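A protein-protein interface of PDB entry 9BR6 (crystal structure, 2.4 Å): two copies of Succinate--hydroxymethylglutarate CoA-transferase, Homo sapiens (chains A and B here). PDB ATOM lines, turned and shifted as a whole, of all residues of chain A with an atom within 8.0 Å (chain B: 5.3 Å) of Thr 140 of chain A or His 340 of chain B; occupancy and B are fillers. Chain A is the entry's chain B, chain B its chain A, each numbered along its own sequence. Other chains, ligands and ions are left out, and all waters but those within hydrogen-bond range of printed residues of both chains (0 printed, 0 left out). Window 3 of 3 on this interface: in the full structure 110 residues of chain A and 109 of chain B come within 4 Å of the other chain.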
ATOM      1  N   PRO A 109      10.692 -13.751  20.217  1.00  0.00           N
ATOM      2  CA  PRO A 109      11.571 -14.504  19.313  1.00  0.00           C
ATOM      3  C   PRO A 109      10.939 -15.816  18.874  1.00  0.00           C
ATOM      4  O   PRO A 109      10.344 -16.541  19.675  1.00  0.00           O
ATOM      5  CB  PRO A 109      12.829 -14.737  20.159  1.00  0.00           C
ATOM      6  CG  PRO A 109      12.844 -13.623  21.124  1.00  0.00           C
ATOM      7  CD  PRO A 109      11.399 -13.331  21.440  1.00  0.00           C
ATOM      8  N   THR A 135      13.155  -6.989  21.436  1.00  0.00           N
ATOM      9  CA  THR A 135      12.527  -7.969  22.308  1.00  0.00           C
ATOM     10  C   THR A 135      12.644  -7.521  23.757  1.00  0.00           C
ATOM     11  O   THR A 135      13.250  -6.496  24.074  1.00  0.00           O
ATOM     12  CB  THR A 135      13.137  -9.364  22.125  1.00  0.00           C
ATOM     13  OG1 THR A 135      14.568  -9.284  22.184  1.00  0.00           O
ATOM     14  CG2 THR A 135      12.728  -9.938  20.777  1.00  0.00           C
ATOM     15  N   TYR A 137      13.983  -9.541  26.277  1.00  0.00           N
ATOM     16  CA  TYR A 137      15.194 -10.058  26.901  1.00  0.00           C
ATOM     17  C   TYR A 137      16.263 -10.576  25.942  1.00  0.00           C
ATOM     18  O   TYR A 137      17.320 -11.011  26.410  1.00  0.00           O
ATOM     19  CB  TYR A 137      14.832 -11.183  27.880  1.00  0.00           C
ATOM     20  CG  TYR A 137      13.741 -10.809  28.852  1.00  0.00           C
ATOM     21  CD1 TYR A 137      14.045 -10.204  30.062  1.00  0.00           C
ATOM     22  CD2 TYR A 137      12.406 -11.058  28.562  1.00  0.00           C
ATOM     23  CE1 TYR A 137      13.050  -9.856  30.957  1.00  0.00           C
ATOM     24  CE2 TYR A 137      11.405 -10.715  29.452  1.00  0.00           C
ATOM     25  CZ  TYR A 137      11.735 -10.115  30.648  1.00  0.00           C
ATOM     26  OH  TYR A 137      10.751  -9.769  31.542  1.00  0.00           O
ATOM     27  N   GLY A 138      16.026 -10.565  24.639  1.00  0.00           N
ATOM     28  CA  GLY A 138      16.993 -11.036  23.667  1.00  0.00           C
ATOM     29  C   GLY A 138      16.488 -12.243  22.893  1.00  0.00           C
ATOM     30  O   GLY A 138      15.517 -12.900  23.262  1.00  0.00           O
ATOM     31  N   GLN A 139      17.213 -12.545  21.813  1.00  0.00           N
ATOM     32  CA  GLN A 139      16.800 -13.627  20.920  1.00  0.00           C
ATOM     33  C   GLN A 139      16.879 -14.986  21.604  1.00  0.00           C
ATOM     34  O   GLN A 139      16.037 -15.859  21.363  1.00  0.00           O
ATOM     35  CB  GLN A 139      17.644 -13.614  19.644  1.00  0.00           C
ATOM     36  CG  GLN A 139      17.270 -12.489  18.690  1.00  0.00           C
ATOM     37  CD  GLN A 139      15.778 -12.434  18.420  1.00  0.00           C
ATOM     38  OE1 GLN A 139      15.126 -11.425  18.687  1.00  0.00           O
ATOM     39  NE2 GLN A 139      15.232 -13.516  17.869  1.00  0.00           N
ATOM     40  N   THR A 140      17.888 -15.195  22.441  1.00  0.00           N
ATOM     41  CA  THR A 140      18.084 -16.468  23.110  1.00  0.00           C
ATOM     42  C   THR A 140      18.329 -16.236  24.596  1.00  0.00           C
ATOM     43  O   THR A 140      18.661 -15.128  25.031  1.00  0.00           O
ATOM     44  CB  THR A 140      19.247 -17.259  22.488  1.00  0.00           C
ATOM     45  OG1 THR A 140      20.430 -16.451  22.479  1.00  0.00           O
ATOM     46  CG2 THR A 140      18.908 -17.671  21.061  1.00  0.00           C
ATOM     47  N   GLY A 141      18.081 -17.285  25.380  1.00  0.00           N
ATOM     48  CA  GLY A 141      18.312 -17.254  26.802  1.00  0.00           C
ATOM     49  C   GLY A 141      17.241 -18.011  27.559  1.00  0.00           C
ATOM     50  O   GLY A 141      16.222 -18.418  26.993  1.00  0.00           O
ATOM     51  N   PRO A 142      17.442 -18.196  28.866  1.00  0.00           N
ATOM     52  CA  PRO A 142      16.416 -18.892  29.663  1.00  0.00           C
ATOM     53  C   PRO A 142      15.088 -18.151  29.751  1.00  0.00           C
ATOM     54  O   PRO A 142      14.040 -18.804  29.783  1.00  0.00           O
ATOM     55  CB  PRO A 142      17.092 -19.057  31.034  1.00  0.00           C
ATOM     56  CG  PRO A 142      18.183 -18.045  31.060  1.00  0.00           C
ATOM     57  CD  PRO A 142      18.661 -17.926  29.645  1.00  0.00           C
ATOM     58  N   ILE A 143      15.089 -16.822  29.835  1.00  0.00           N
ATOM     59  CA  ILE A 143      13.846 -16.056  29.930  1.00  0.00           C
ATOM     60  C   ILE A 143      13.526 -15.322  28.622  1.00  0.00           C
ATOM     61  O   ILE A 143      12.723 -14.388  28.616  1.00  0.00           O
ATOM     62  CB  ILE A 143      13.872 -15.085  31.123  1.00  0.00           C
ATOM     63  CG1 ILE A 143      14.961 -14.030  30.940  1.00  0.00           C
ATOM     64  CG2 ILE A 143      14.071 -15.842  32.423  1.00  0.00           C
ATOM     65  CD1 ILE A 143      15.090 -13.081  32.109  1.00  0.00           C
ATOM     66  N   SER A 144      14.142 -15.734  27.512  1.00  0.00           N
ATOM     67  CA  SER A 144      13.947 -15.054  26.233  1.00  0.00           C
ATOM     68  C   SER A 144      12.509 -15.151  25.722  1.00  0.00           C
ATOM     69  O   SER A 144      12.045 -14.251  25.012  1.00  0.00           O
ATOM     70  CB  SER A 144      14.934 -15.609  25.202  1.00  0.00           C
ATOM     71  OG  SER A 144      14.607 -16.933  24.818  1.00  0.00           O
ATOM     72  N   GLN A 145      11.803 -16.242  26.032  1.00  0.00           N
ATOM     73  CA  GLN A 145      10.436 -16.424  25.547  1.00  0.00           C
ATOM     74  C   GLN A 145       9.428 -15.483  26.206  1.00  0.00           C
ATOM     75  O   GLN A 145       8.337 -15.288  25.659  1.00  0.00           O
ATOM     76  CB  GLN A 145      10.007 -17.881  25.734  1.00  0.00           C
ATOM     77  CG  GLN A 145      10.537 -18.816  24.645  1.00  0.00           C
ATOM     78  CD  GLN A 145      10.123 -18.395  23.240  1.00  0.00           C
ATOM     79  OE1 GLN A 145       8.939 -18.410  22.896  1.00  0.00           O
ATOM     80  NE2 GLN A 145      11.100 -18.002  22.428  1.00  0.00           N
ATOM     81  N   ASP A 207      20.088  -7.471  17.132  1.00  0.00           N
ATOM     82  CA  ASP A 207      19.362  -7.850  18.338  1.00  0.00           C
ATOM     83  C   ASP A 207      19.335  -6.655  19.285  1.00  0.00           C
ATOM     84  O   ASP A 207      20.389  -6.164  19.703  1.00  0.00           O
ATOM     85  CB  ASP A 207      19.991  -9.074  19.007  1.00  0.00           C
ATOM     86  CG  ASP A 207      19.206  -9.552  20.230  1.00  0.00           C
ATOM     87  OD1 ASP A 207      18.198  -8.907  20.600  1.00  0.00           O
ATOM     88  OD2 ASP A 207      19.590 -10.591  20.813  1.00  0.00           O
ATOM     89  N   ASN A 209      17.163  -5.410  22.859  1.00  0.00           N
ATOM     90  CA  ASN A 209      16.220  -5.838  23.877  1.00  0.00           C
ATOM     91  C   ASN A 209      16.212  -4.854  25.038  1.00  0.00           C
ATOM     92  O   ASN A 209      17.191  -4.142  25.285  1.00  0.00           O
ATOM     93  CB  ASN A 209      16.531  -7.254  24.373  1.00  0.00           C
ATOM     94  CG  ASN A 209      17.900  -7.361  25.006  1.00  0.00           C
ATOM     95  OD1 ASN A 209      18.027  -7.331  26.227  1.00  0.00           O
ATOM     96  ND2 ASN A 209      18.934  -7.478  24.176  1.00  0.00           N
ATOM     97  N   LEU A 211      16.169  -5.493  28.272  1.00  0.00           N
ATOM     98  CA  LEU A 211      17.059  -5.851  29.373  1.00  0.00           C
ATOM     99  C   LEU A 211      18.473  -5.344  29.120  1.00  0.00           C
ATOM    100  O   LEU A 211      19.088  -4.719  29.991  1.00  0.00           O
ATOM    101  CB  LEU A 211      17.051  -7.366  29.585  1.00  0.00           C
ATOM    102  CG  LEU A 211      17.993  -7.900  30.668  1.00  0.00           C
ATOM    103  CD1 LEU A 211      17.613  -7.355  32.034  1.00  0.00           C
ATOM    104  CD2 LEU A 211      18.004  -9.422  30.683  1.00  0.00           C
ATOM    105  N   SER A 212      18.999  -5.588  27.918  1.00  0.00           N
ATOM    106  CA  SER A 212      20.346  -5.126  27.601  1.00  0.00           C
ATOM    107  C   SER A 212      20.428  -3.604  27.612  1.00  0.00           C
ATOM    108  O   SER A 212      21.413  -3.037  28.100  1.00  0.00           O
ATOM    109  CB  SER A 212      20.792  -5.689  26.251  1.00  0.00           C
ATOM    110  OG  SER A 212      21.060  -7.084  26.343  1.00  0.00           O
ATOM    111  N   PRO B 336      21.029 -15.296  35.028  1.00  0.00           N
ATOM    112  CA  PRO B 336      21.753 -15.891  33.891  1.00  0.00           C
ATOM    113  C   PRO B 336      21.503 -15.175  32.573  1.00  0.00           C
ATOM    114  O   PRO B 336      22.420 -15.093  31.746  1.00  0.00           O
ATOM    115  CB  PRO B 336      21.229 -17.334  33.861  1.00  0.00           C
ATOM    116  CG  PRO B 336      20.737 -17.588  35.262  1.00  0.00           C
ATOM    117  CD  PRO B 336      20.172 -16.275  35.717  1.00  0.00           C
ATOM    118  N   GLN B 337      20.292 -14.654  32.353  1.00  0.00           N
ATOM    119  CA  GLN B 337      20.009 -13.945  31.106  1.00  0.00           C
ATOM    120  C   GLN B 337      20.923 -12.738  30.932  1.00  0.00           C
ATOM    121  O   GLN B 337      21.390 -12.461  29.821  1.00  0.00           O
ATOM    122  CB  GLN B 337      18.543 -13.517  31.067  1.00  0.00           C
ATOM    123  CG  GLN B 337      18.103 -12.919  29.737  1.00  0.00           C
ATOM    124  CD  GLN B 337      17.951 -13.959  28.646  1.00  0.00           C
ATOM    125  OE1 GLN B 337      17.279 -14.972  28.827  1.00  0.00           O
ATOM    126  NE2 GLN B 337      18.573 -13.708  27.500  1.00  0.00           N
ATOM    127  N   VAL B 338      21.196 -12.009  32.019  1.00  0.00           N
ATOM    128  CA  VAL B 338      22.101 -10.863  31.942  1.00  0.00           C
ATOM    129  C   VAL B 338      23.492 -11.308  31.511  1.00  0.00           C
ATOM    130  O   VAL B 338      24.134 -10.665  30.669  1.00  0.00           O
ATOM    131  CB  VAL B 338      22.138 -10.114  33.288  1.00  0.00           C
ATOM    132  CG1 VAL B 338      23.307  -9.145  33.323  1.00  0.00           C
ATOM    133  CG2 VAL B 338      20.826  -9.367  33.512  1.00  0.00           C
ATOM    134  N   LEU B 339      23.982 -12.415  32.073  1.00  0.00           N
ATOM    135  CA  LEU B 339      25.288 -12.920  31.666  1.00  0.00           C
ATOM    136  C   LEU B 339      25.260 -13.411  30.226  1.00  0.00           C
ATOM    137  O   LEU B 339      26.180 -13.125  29.451  1.00  0.00           O
ATOM    138  CB  LEU B 339      25.728 -14.043  32.604  1.00  0.00           C
ATOM    139  CG  LEU B 339      25.766 -13.676  34.086  1.00  0.00           C
ATOM    140  CD1 LEU B 339      26.183 -14.873  34.907  1.00  0.00           C
ATOM    141  CD2 LEU B 339      26.711 -12.513  34.316  1.00  0.00           C
ATOM    142  N   HIS B 340      24.186 -14.109  29.844  1.00  0.00           N
ATOM    143  CA  HIS B 340      24.080 -14.667  28.499  1.00  0.00           C
ATOM    144  C   HIS B 340      24.114 -13.576  27.437  1.00  0.00           C
ATOM    145  O   HIS B 340      24.660 -13.777  26.347  1.00  0.00           O
ATOM    146  CB  HIS B 340      22.794 -15.487  28.386  1.00  0.00           C
ATOM    147  CG  HIS B 340      22.511 -15.990  27.005  1.00  0.00           C
ATOM    148  ND1 HIS B 340      22.981 -17.203  26.542  1.00  0.00           N
ATOM    149  CD2 HIS B 340      21.797 -15.452  25.988  1.00  0.00           C
ATOM    150  CE1 HIS B 340      22.571 -17.386  25.301  1.00  0.00           C
ATOM    151  NE2 HIS B 340      21.851 -16.337  24.940  1.00  0.00           N
ATOM    152  N   ASN B 341      23.533 -12.411  27.737  1.00  0.00           N
ATOM    153  CA  ASN B 341      23.533 -11.287  26.804  1.00  0.00           C
ATOM    154  C   ASN B 341      24.893 -10.606  26.690  1.00  0.00           C
ATOM    155  O   ASN B 341      25.027  -9.665  25.898  1.00  0.00           O
ATOM    156  CB  ASN B 341      22.474 -10.261  27.211  1.00  0.00           C
ATOM    157  CG  ASN B 341      21.065 -10.704  26.863  1.00  0.00           C
ATOM    158  OD1 ASN B 341      20.834 -11.854  26.492  1.00  0.00           O
ATOM    159  ND2 ASN B 341      20.117  -9.781  26.958  1.00  0.00           N
ATOM    160  N   GLY B 342      25.885 -11.029  27.471  1.00  0.00           N
ATOM    161  CA  GLY B 342      27.194 -10.412  27.418  1.00  0.00           C
ATOM    162  C   GLY B 342      27.291  -9.117  28.182  1.00  0.00           C
ATOM    163  O   GLY B 342      28.268  -8.381  28.011  1.00  0.00           O
ATOM    164  N   ARG B 363      23.698  -6.425  19.946  1.00  0.00           N
ATOM    165  CA  ARG B 363      24.539  -7.486  19.402  1.00  0.00           C
ATOM    166  C   ARG B 363      24.221  -7.661  17.922  1.00  0.00           C
ATOM    167  O   ARG B 363      23.047  -7.729  17.541  1.00  0.00           O
ATOM    168  CB  ARG B 363      24.330  -8.804  20.158  1.00  0.00           C
ATOM    169  CG  ARG B 363      24.921  -8.825  21.568  1.00  0.00           C
ATOM    170  CD  ARG B 363      24.398 -10.017  22.367  1.00  0.00           C
ATOM    171  NE  ARG B 363      22.967  -9.884  22.612  1.00  0.00           N
ATOM    172  CZ  ARG B 363      22.186 -10.842  23.094  1.00  0.00           C
ATOM    173  NH1 ARG B 363      22.664 -12.036  23.401  1.00  0.00           N
ATOM    174  NH2 ARG B 363      20.890 -10.597  23.263  1.00  0.00           N
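NE2 of Gln 337 of chain B is in hydrogen-bond range of O of Tyr 137 of chain A, 3.2 Å away.
The backbone carbonyl oxygen (O) of Thr 140 of chain A sits at hydrogen-bond distance from the side-chain amide nitrogen (NE2) of Gln 337 of chain B (2.8 Å).
The side-chain amide oxygen of Gln 337 of chain B is in hydrogen-bond range of the backbone NH of Ile 143 of chain A (3.0 Å).
The side-chain amide oxygen (OE1) of Gln 337 of chain B lies within hydrogen-bond range of the backbone NH (N) of Ser 144 of chain A.
OG1 of Thr 140 of chain A is in hydrogen-bond range of NE2 of His 340 of chain B, 2.8 Å away.
The backbone carbonyl oxygen (O) of Tyr 137 of chain A is in hydrogen-bond range of the side-chain amide nitrogen (ND2) of Asn 341 of chain B, at 3.1 Å.
The side-chain amide oxygen (OD1) of Asn 209 of chain A sits at hydrogen-bond distance from the side-chain amide nitrogen (ND2) of Asn 341 of chain B.
The side-chain amide nitrogen (ND2) of Asn 341 of chain B sits at hydrogen-bond distance from the side-chain hydroxyl (OG) of Ser 212 of chain A, at 2.9 Å.
The guanidinium group (NH2) of Arg 363 of chain B lies within salt-bridge range of the side-chain carboxylate (OD2) of Asp 207 of chain A (2.8 Å).
OE1 of Gln 337 of chain B lies close to N of Pro 142 of chain A (3.2 Å).
Among the printed residues, merely in contact across the chains: Gly 141 of chain A with Gln 337 of chain B (3.2 Å), Leu 211 of chain A with Gln 337 of chain B (3.6 Å), Asn 209 of chain A with Arg 363 of chain B (3.8 Å), Gly 141 of chain A with His 340 of chain B (3.9 Å), Gly 138 of chain A with Arg 363 of chain B (3.9 Å) and Leu 211 of chain A with Val 338 of chain B (3.996 Å).
The side-chain amide nitrogen of Gln 337 of chain B lies within hydrogen-bond range of the side-chain amide oxygen of Asn 341 of chain B (3.1 Å).
The side-chain amide oxygen (OD1) of Asn 341 of chain B sits at hydrogen-bond distance from the guanidinium group (NH2) of Arg 363 of chain B (3.5 Å).
N of Gly 138 of chain A lies within hydrogen-bond range of OG1 of Thr 135 of chain A (3.1 Å).
N of Gln 139 of chain A lies within hydrogen-bond range of OD2 of Asp 207 of chain A.
The backbone carbonyl oxygen (O) of Gly 141 of chain A is in hydrogen-bond range of the side-chain hydroxyl (OG) of Ser 144 of chain A, at 3.1 Å.
The side-chain amide oxygen (OD1) of Asn 209 of chain A lies close to the backbone NH (N) of Leu 211 of chain A (3.3 Å).
No position is printed for both chains.
Of the 16 pairs that touch across the chains among the printed residues, none has its exchanged pair printed and touching as well.
Of the 15 printed residues of chain A, 11 touch a printed residue of chain B.
Among the printed residues, 16 pairs touch across the chains.
Among the printed residues, Asp or Glu carboxylates within 4 Å of a Lys or Arg side-chain nitrogen of the other chain: Asp 207 of chain A with Arg 363 of chain B.
Of the printed residues of chain B, Tyr 137 of chain A touches Gln 337 (3.2 Å) and Asn 341 (3.1 Å).
Thr 140 of chain A touches just these residues of chain B: Gln 337 (2.8 Å) and His 340 (2.8 Å).
Gln 145 of chain A touches none of the printed residues of chain B.
Of the printed residues of chain B, Asp 207 of chain A touches Arg 363.
The nearest residue of chain B that does not touch Thr 140 of chain A is Asn 341 of chain B (4.2 Å).
The nearest residue of chain A that does not touch His 340 of chain B is Pro 142 of chain A (5.0 Å).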
